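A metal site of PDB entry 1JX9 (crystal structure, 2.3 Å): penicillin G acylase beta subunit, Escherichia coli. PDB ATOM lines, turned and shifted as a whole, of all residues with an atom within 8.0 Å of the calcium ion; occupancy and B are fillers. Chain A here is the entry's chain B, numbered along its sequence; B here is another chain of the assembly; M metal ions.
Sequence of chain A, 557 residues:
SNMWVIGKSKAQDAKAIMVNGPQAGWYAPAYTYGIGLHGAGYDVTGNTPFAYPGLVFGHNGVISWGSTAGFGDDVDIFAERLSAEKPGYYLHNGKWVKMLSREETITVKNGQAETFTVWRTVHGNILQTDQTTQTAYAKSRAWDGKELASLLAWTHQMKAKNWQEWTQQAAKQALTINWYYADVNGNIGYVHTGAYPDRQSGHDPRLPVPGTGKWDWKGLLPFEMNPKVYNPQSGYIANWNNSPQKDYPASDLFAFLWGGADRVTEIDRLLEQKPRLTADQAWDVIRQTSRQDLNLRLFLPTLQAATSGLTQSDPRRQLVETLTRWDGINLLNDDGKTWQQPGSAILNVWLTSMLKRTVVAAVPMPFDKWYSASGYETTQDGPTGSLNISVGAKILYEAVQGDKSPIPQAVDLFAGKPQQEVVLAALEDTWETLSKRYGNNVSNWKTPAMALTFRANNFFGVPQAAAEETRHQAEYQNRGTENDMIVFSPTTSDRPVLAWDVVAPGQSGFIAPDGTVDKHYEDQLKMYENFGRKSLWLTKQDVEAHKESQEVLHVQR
The guanidinium group (NH2) of Arg 199 is in hydrogen-bond range of the backbone carbonyl oxygen (O) of Asp 73 (3.1 Å).
The backbone carbonyl oxygen (O) of Asp 252 lies within hydrogen-bond range of the side-chain amide nitrogen (ND2) of Asn 156 of chain B (2.6 Å).
The side-chain hydroxyl (OG1) of Thr 151 of chain B lies within hydrogen-bond range of the side-chain carboxylate (OD1) of Asp 252 (3.0 Å).
The backbone NH (N) of Glu 153 of chain B sits at hydrogen-bond distance from the side-chain hydroxyl (OG1) of Thr 151 of chain B, 3.5 Å away.
The backbone NH (N) of Ser 140 is in hydrogen-bond range of the backbone carbonyl oxygen (O) of Asp 76.
The side-chain carboxylate (OD2) of Asp 76 is in hydrogen-bond range of the indole nitrogen (NE1) of Trp 217, 2.7 Å away.
The side-chain carboxylate (OE1) of Glu 153 of chain B lies within hydrogen-bond range of the backbone NH (N) of Ile 77.
NE of Arg 199 lies within salt-bridge range of OD2 of Asp 76, at 2.6 Å.
Residues that only touch the calcium ion: Arg 199 (3.97 Å).
Within 4 Å of the calcium ion: Asp 73, Val 75, Asp 76, Arg 199, Pro 205, Asp 252 and Glu 153 of chain B.
The nearest printed residue that does not touch the calcium ion is Thr 151 of chain B (4.6 Å).
The calcium ion is bound by the side-chain carboxylate (OE2) of Glu 153 of chain B (2.2 Å), the backbone carbonyl oxygen (O) of Val 75 (2.3 Å), the side-chain carboxylate (OD2) of Asp 252 (2.4 Å), the side-chain carboxylate (OD1) of Asp 76 (2.5 Å), the backbone carbonyl oxygen (O) of Pro 205 (2.6 Å), the side-chain carboxylate (OD1) of Asp 73 (2.6 Å) and the side-chain carboxylate (OD2) of Asp 73 (2.6 Å).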
ATOM      1  N   GLY A  72       7.725  17.852 -34.133  1.00  0.00           N
ATOM      2  CA  GLY A  72       9.089  18.023 -33.680  1.00  0.00           C
ATOM      3  C   GLY A  72       9.266  16.992 -32.571  1.00  0.00           C
ATOM      4  O   GLY A  72       8.265  16.405 -32.123  1.00  0.00           O
ATOM      5  N   ASP A  73      10.496  16.750 -32.120  1.00  0.00           N
ATOM      6  CA  ASP A  73      10.713  15.779 -31.041  1.00  0.00           C
ATOM      7  C   ASP A  73      10.618  16.432 -29.669  1.00  0.00           C
ATOM      8  O   ASP A  73      11.587  16.982 -29.149  1.00  0.00           O
ATOM      9  CB  ASP A  73      12.080  15.106 -31.192  1.00  0.00           C
ATOM     10  CG  ASP A  73      12.275  13.943 -30.224  1.00  0.00           C
ATOM     11  OD1 ASP A  73      11.503  13.792 -29.246  1.00  0.00           O
ATOM     12  OD2 ASP A  73      13.220  13.144 -30.360  1.00  0.00           O
ATOM     13  N   ASP A  74       9.439  16.363 -29.063  1.00  0.00           N
ATOM     14  CA  ASP A  74       9.277  16.987 -27.755  1.00  0.00           C
ATOM     15  C   ASP A  74       8.981  15.955 -26.645  1.00  0.00           C
ATOM     16  O   ASP A  74       8.485  16.300 -25.581  1.00  0.00           O
ATOM     17  CB  ASP A  74       8.192  18.060 -27.829  1.00  0.00           C
ATOM     18  CG  ASP A  74       6.828  17.478 -28.087  1.00  0.00           C
ATOM     19  OD1 ASP A  74       6.742  16.258 -28.271  1.00  0.00           O
ATOM     20  OD2 ASP A  74       5.778  18.157 -28.114  1.00  0.00           O
ATOM     21  N   VAL A  75       9.318  14.690 -26.917  1.00  0.00           N
ATOM     22  CA  VAL A  75       9.091  13.602 -25.972  1.00  0.00           C
ATOM     23  C   VAL A  75      10.303  12.643 -25.900  1.00  0.00           C
ATOM     24  O   VAL A  75      10.789  12.164 -26.905  1.00  0.00           O
ATOM     25  CB  VAL A  75       7.854  12.775 -26.369  1.00  0.00           C
ATOM     26  CG1 VAL A  75       7.595  11.677 -25.334  1.00  0.00           C
ATOM     27  CG2 VAL A  75       6.602  13.671 -26.542  1.00  0.00           C
ATOM     28  N   ASP A  76      10.788  12.386 -24.697  1.00  0.00           N
ATOM     29  CA  ASP A  76      11.854  11.425 -24.529  1.00  0.00           C
ATOM     30  C   ASP A  76      11.398  10.432 -23.504  1.00  0.00           C
ATOM     31  O   ASP A  76      10.559  10.735 -22.661  1.00  0.00           O
ATOM     32  CB  ASP A  76      13.151  12.105 -24.050  1.00  0.00           C
ATOM     33  CG  ASP A  76      13.762  13.019 -25.084  1.00  0.00           C
ATOM     34  OD1 ASP A  76      13.438  12.889 -26.303  1.00  0.00           O
ATOM     35  OD2 ASP A  76      14.564  13.937 -24.755  1.00  0.00           O
ATOM     36  N   ILE A  77      11.976   9.237 -23.556  1.00  0.00           N
ATOM     37  CA  ILE A  77      11.621   8.184 -22.614  1.00  0.00           C
ATOM     38  C   ILE A  77      12.771   7.926 -21.659  1.00  0.00           C
ATOM     39  O   ILE A  77      13.910   7.740 -22.079  1.00  0.00           O
ATOM     40  CB  ILE A  77      11.233   6.924 -23.411  1.00  0.00           C
ATOM     41  CG1 ILE A  77       9.928   7.197 -24.193  1.00  0.00           C
ATOM     42  CG2 ILE A  77      11.114   5.711 -22.499  1.00  0.00           C
ATOM     43  CD1 ILE A  77       9.326   5.954 -24.843  1.00  0.00           C
ATOM     44  N   SER A 140       8.439  11.260 -21.039  1.00  0.00           N
ATOM     45  CA  SER A 140       8.702  12.623 -20.624  1.00  0.00           C
ATOM     46  C   SER A 140       8.386  13.581 -21.743  1.00  0.00           C
ATOM     47  O   SER A 140       9.033  13.552 -22.793  1.00  0.00           O
ATOM     48  CB  SER A 140      10.174  12.767 -20.217  1.00  0.00           C
ATOM     49  OG  SER A 140      10.397  14.020 -19.648  1.00  0.00           O
ATOM     50  N   PRO A 197      13.119  20.138 -25.176  1.00  0.00           N
ATOM     51  CA  PRO A 197      14.074  19.976 -24.073  1.00  0.00           C
ATOM     52  C   PRO A 197      15.476  20.329 -24.459  1.00  0.00           C
ATOM     53  O   PRO A 197      15.876  20.188 -25.610  1.00  0.00           O
ATOM     54  CB  PRO A 197      13.960  18.484 -23.749  1.00  0.00           C
ATOM     55  CG  PRO A 197      13.624  17.872 -25.072  1.00  0.00           C
ATOM     56  CD  PRO A 197      12.639  18.836 -25.680  1.00  0.00           C
ATOM     57  N   ARG A 199      18.685  19.055 -23.965  1.00  0.00           N
ATOM     58  CA  ARG A 199      19.253  17.762 -23.650  1.00  0.00           C
ATOM     59  C   ARG A 199      20.739  17.788 -23.341  1.00  0.00           C
ATOM     60  O   ARG A 199      21.478  18.619 -23.883  1.00  0.00           O
ATOM     61  CB  ARG A 199      18.974  16.785 -24.808  1.00  0.00           C
ATOM     62  CG  ARG A 199      17.472  16.521 -25.087  1.00  0.00           C
ATOM     63  CD  ARG A 199      17.225  15.681 -26.349  1.00  0.00           C
ATOM     64  NE  ARG A 199      15.838  15.291 -26.610  1.00  0.00           N
ATOM     65  CZ  ARG A 199      15.026  15.880 -27.491  1.00  0.00           C
ATOM     66  NH1 ARG A 199      15.407  16.945 -28.213  1.00  0.00           N
ATOM     67  NH2 ARG A 199      13.805  15.402 -27.656  1.00  0.00           N
ATOM     68  N   HIS A 203      23.266  13.004 -25.701  1.00  0.00           N
ATOM     69  CA  HIS A 203      21.907  12.436 -25.669  1.00  0.00           C
ATOM     70  C   HIS A 203      21.328  12.299 -27.066  1.00  0.00           C
ATOM     71  O   HIS A 203      21.029  13.286 -27.720  1.00  0.00           O
ATOM     72  CB  HIS A 203      21.009  13.314 -24.779  1.00  0.00           C
ATOM     73  CG  HIS A 203      19.578  12.855 -24.675  1.00  0.00           C
ATOM     74  ND1 HIS A 203      18.733  13.338 -23.702  1.00  0.00           N
ATOM     75  CD2 HIS A 203      18.853  11.986 -25.417  1.00  0.00           C
ATOM     76  CE1 HIS A 203      17.535  12.797 -23.856  1.00  0.00           C
ATOM     77  NE2 HIS A 203      17.585  11.965 -24.888  1.00  0.00           N
ATOM     78  N   ASP A 204      21.178  11.071 -27.543  1.00  0.00           N
ATOM     79  CA  ASP A 204      20.612  10.820 -28.881  1.00  0.00           C
ATOM     80  C   ASP A 204      19.094  10.751 -28.678  1.00  0.00           C
ATOM     81  O   ASP A 204      18.604   9.788 -28.100  1.00  0.00           O
ATOM     82  CB  ASP A 204      21.181   9.492 -29.427  1.00  0.00           C
ATOM     83  CG  ASP A 204      20.653   9.122 -30.810  1.00  0.00           C
ATOM     84  OD1 ASP A 204      19.464   9.396 -31.118  1.00  0.00           O
ATOM     85  OD2 ASP A 204      21.382   8.486 -31.636  1.00  0.00           O
ATOM     86  N   PRO A 205      18.368  11.758 -29.169  1.00  0.00           N
ATOM     87  CA  PRO A 205      16.935  11.934 -28.881  1.00  0.00           C
ATOM     88  C   PRO A 205      16.021  10.901 -29.570  1.00  0.00           C
ATOM     89  O   PRO A 205      14.824  10.957 -29.448  1.00  0.00           O
ATOM     90  CB  PRO A 205      16.655  13.337 -29.405  1.00  0.00           C
ATOM     91  CG  PRO A 205      17.627  13.458 -30.573  1.00  0.00           C
ATOM     92  CD  PRO A 205      18.887  12.818 -30.053  1.00  0.00           C
ATOM     93  N   ARG A 206      16.615   9.952 -30.278  1.00  0.00           N
ATOM     94  CA  ARG A 206      15.836   8.939 -30.918  1.00  0.00           C
ATOM     95  C   ARG A 206      15.779   7.701 -30.034  1.00  0.00           C
ATOM     96  O   ARG A 206      15.082   6.758 -30.339  1.00  0.00           O
ATOM     97  CB  ARG A 206      16.483   8.554 -32.250  1.00  0.00           C
ATOM     98  CG  ARG A 206      16.606   9.695 -33.223  1.00  0.00           C
ATOM     99  CD  ARG A 206      17.449   9.337 -34.405  1.00  0.00           C
ATOM    100  NE  ARG A 206      18.776   8.952 -33.956  1.00  0.00           N
ATOM    101  CZ  ARG A 206      19.755   8.596 -34.773  1.00  0.00           C
ATOM    102  NH1 ARG A 206      19.537   8.569 -36.091  1.00  0.00           N
ATOM    103  NH2 ARG A 206      20.935   8.262 -34.259  1.00  0.00           N
ATOM    104  N   LEU A 207      16.509   7.711 -28.919  1.00  0.00           N
ATOM    105  CA  LEU A 207      16.577   6.525 -28.080  1.00  0.00           C
ATOM    106  C   LEU A 207      16.410   6.844 -26.594  1.00  0.00           C
ATOM    107  O   LEU A 207      16.707   7.950 -26.174  1.00  0.00           O
ATOM    108  CB  LEU A 207      17.905   5.810 -28.347  1.00  0.00           C
ATOM    109  CG  LEU A 207      18.067   5.422 -29.817  1.00  0.00           C
ATOM    110  CD1 LEU A 207      19.462   4.925 -30.163  1.00  0.00           C
ATOM    111  CD2 LEU A 207      17.043   4.369 -30.203  1.00  0.00           C
ATOM    112  N   PRO A 208      15.951   5.879 -25.802  1.00  0.00           N
ATOM    113  CA  PRO A 208      15.741   6.134 -24.373  1.00  0.00           C
ATOM    114  C   PRO A 208      17.025   6.491 -23.622  1.00  0.00           C
ATOM    115  O   PRO A 208      18.128   6.182 -24.063  1.00  0.00           O
ATOM    116  CB  PRO A 208      15.173   4.801 -23.849  1.00  0.00           C
ATOM    117  CG  PRO A 208      14.643   4.070 -25.092  1.00  0.00           C
ATOM    118  CD  PRO A 208      15.573   4.519 -26.196  1.00  0.00           C
ATOM    119  N   TRP A 217      16.955  16.202 -18.487  1.00  0.00           N
ATOM    120  CA  TRP A 217      17.025  17.365 -19.341  1.00  0.00           C
ATOM    121  C   TRP A 217      17.574  18.533 -18.535  1.00  0.00           C
ATOM    122  O   TRP A 217      17.349  18.605 -17.321  1.00  0.00           O
ATOM    123  CB  TRP A 217      15.633  17.746 -19.820  1.00  0.00           C
ATOM    124  CG  TRP A 217      14.975  16.773 -20.770  1.00  0.00           C
ATOM    125  CD1 TRP A 217      15.582  15.868 -21.583  1.00  0.00           C
ATOM    126  CD2 TRP A 217      13.577  16.688 -21.039  1.00  0.00           C
ATOM    127  NE1 TRP A 217      14.638  15.198 -22.324  1.00  0.00           N
ATOM    128  CE2 TRP A 217      13.398  15.678 -22.006  1.00  0.00           C
ATOM    129  CE3 TRP A 217      12.454  17.353 -20.546  1.00  0.00           C
ATOM    130  CZ2 TRP A 217      12.147  15.338 -22.496  1.00  0.00           C
ATOM    131  CZ3 TRP A 217      11.222  17.002 -21.011  1.00  0.00           C
ATOM    132  CH2 TRP A 217      11.072  15.998 -21.985  1.00  0.00           C
ATOM    133  N   ALA A 250      13.242  15.798 -36.682  1.00  0.00           N
ATOM    134  CA  ALA A 250      11.881  15.311 -36.577  1.00  0.00           C
ATOM    135  C   ALA A 250      11.597  14.532 -35.322  1.00  0.00           C
ATOM    136  O   ALA A 250      12.487  14.196 -34.528  1.00  0.00           O
ATOM    137  CB  ALA A 250      11.548  14.449 -37.784  1.00  0.00           C
ATOM    138  N   SER A 251      10.323  14.196 -35.202  1.00  0.00           N
ATOM    139  CA  SER A 251       9.816  13.324 -34.178  1.00  0.00           C
ATOM    140  C   SER A 251      10.618  12.041 -34.252  1.00  0.00           C
ATOM    141  O   SER A 251      11.048  11.651 -35.340  1.00  0.00           O
ATOM    142  CB  SER A 251       8.353  13.022 -34.475  1.00  0.00           C
ATOM    143  OG  SER A 251       7.901  11.945 -33.678  1.00  0.00           O
ATOM    144  N   ASP A 252      10.832  11.392 -33.106  1.00  0.00           N
ATOM    145  CA  ASP A 252      11.598  10.144 -33.064  1.00  0.00           C
ATOM    146  C   ASP A 252      10.840   8.932 -33.581  1.00  0.00           C
ATOM    147  O   ASP A 252      11.409   7.855 -33.712  1.00  0.00           O
ATOM    148  CB  ASP A 252      12.194   9.868 -31.665  1.00  0.00           C
ATOM    149  CG  ASP A 252      11.130   9.699 -30.599  1.00  0.00           C
ATOM    150  OD1 ASP A 252      10.166   8.945 -30.814  1.00  0.00           O
ATOM    151  OD2 ASP A 252      11.174  10.289 -29.513  1.00  0.00           O
ATOM    152  N   LEU A 253       9.562   9.116 -33.924  1.00  0.00           N
ATOM    153  CA  LEU A 253       8.751   8.025 -34.503  1.00  0.00           C
ATOM    154  C   LEU A 253       9.480   7.290 -35.618  1.00  0.00           C
ATOM    155  O   LEU A 253       9.831   7.895 -36.604  1.00  0.00           O
ATOM    156  CB  LEU A 253       7.464   8.570 -35.101  1.00  0.00           C
ATOM    157  CG  LEU A 253       6.329   8.892 -34.154  1.00  0.00           C
ATOM    158  CD1 LEU A 253       5.117   9.407 -34.929  1.00  0.00           C
ATOM    159  CD2 LEU A 253       5.961   7.662 -33.379  1.00  0.00           C
ATOM    160  N   SER B 150       3.887  12.011 -29.406  1.00  0.00           N
ATOM    161  CA  SER B 150       4.382  10.925 -30.247  1.00  0.00           C
ATOM    162  C   SER B 150       5.819  10.500 -29.949  1.00  0.00           C
ATOM    163  O   SER B 150       6.728  11.339 -29.973  1.00  0.00           O
ATOM    164  CB  SER B 150       4.339  11.341 -31.721  1.00  0.00           C
ATOM    165  OG  SER B 150       3.025  11.668 -32.118  1.00  0.00           O
ATOM    166  N   THR B 151       6.021   9.213 -29.695  1.00  0.00           N
ATOM    167  CA  THR B 151       7.356   8.650 -29.484  1.00  0.00           C
ATOM    168  C   THR B 151       7.353   7.145 -29.722  1.00  0.00           C
ATOM    169  O   THR B 151       6.330   6.485 -29.519  1.00  0.00           O
ATOM    170  CB  THR B 151       7.861   8.937 -28.082  1.00  0.00           C
ATOM    171  OG1 THR B 151       9.245   8.575 -27.971  1.00  0.00           O
ATOM    172  CG2 THR B 151       7.163   8.016 -27.056  1.00  0.00           C
ATOM    173  N   SER B 152       8.496   6.610 -30.145  1.00  0.00           N
ATOM    174  CA  SER B 152       8.663   5.163 -30.327  1.00  0.00           C
ATOM    175  C   SER B 152      10.098   4.799 -29.942  1.00  0.00           C
ATOM    176  O   SER B 152      10.675   3.858 -30.470  1.00  0.00           O
ATOM    177  CB  SER B 152       8.364   4.728 -31.768  1.00  0.00           C
ATOM    178  OG  SER B 152       9.260   5.303 -32.718  1.00  0.00           O
ATOM    179  N   GLU B 153      10.656   5.555 -29.020  1.00  0.00           N
ATOM    180  CA  GLU B 153      12.040   5.351 -28.603  1.00  0.00           C
ATOM    181  C   GLU B 153      12.352   3.914 -28.187  1.00  0.00           C
ATOM    182  O   GLU B 153      13.430   3.408 -28.487  1.00  0.00           O
ATOM    183  CB  GLU B 153      12.415   6.314 -27.502  1.00  0.00           C
ATOM    184  CG  GLU B 153      12.684   7.713 -28.002  1.00  0.00           C
ATOM    185  CD  GLU B 153      13.128   8.591 -26.892  1.00  0.00           C
ATOM    186  OE1 GLU B 153      13.416   8.019 -25.816  1.00  0.00           O
ATOM    187  OE2 GLU B 153      13.184   9.831 -27.068  1.00  0.00           O
ATOM    188  N   ASN B 156      12.530   1.998 -31.358  1.00  0.00           N
ATOM    189  CA  ASN B 156      13.718   2.441 -32.051  1.00  0.00           C
ATOM    190  C   ASN B 156      14.968   1.714 -31.491  1.00  0.00           C
ATOM    191  O   ASN B 156      15.803   1.269 -32.271  1.00  0.00           O
ATOM    192  CB  ASN B 156      13.890   3.952 -31.931  1.00  0.00           C
ATOM    193  CG  ASN B 156      12.775   4.743 -32.616  1.00  0.00           C
ATOM    194  OD1 ASN B 156      11.925   4.190 -33.334  1.00  0.00           O
ATOM    195  ND2 ASN B 156      12.776   6.053 -32.390  1.00  0.00           N
HETATM  196 CA    CA M   1      12.636  11.656 -28.264  1.00  0.00          CA
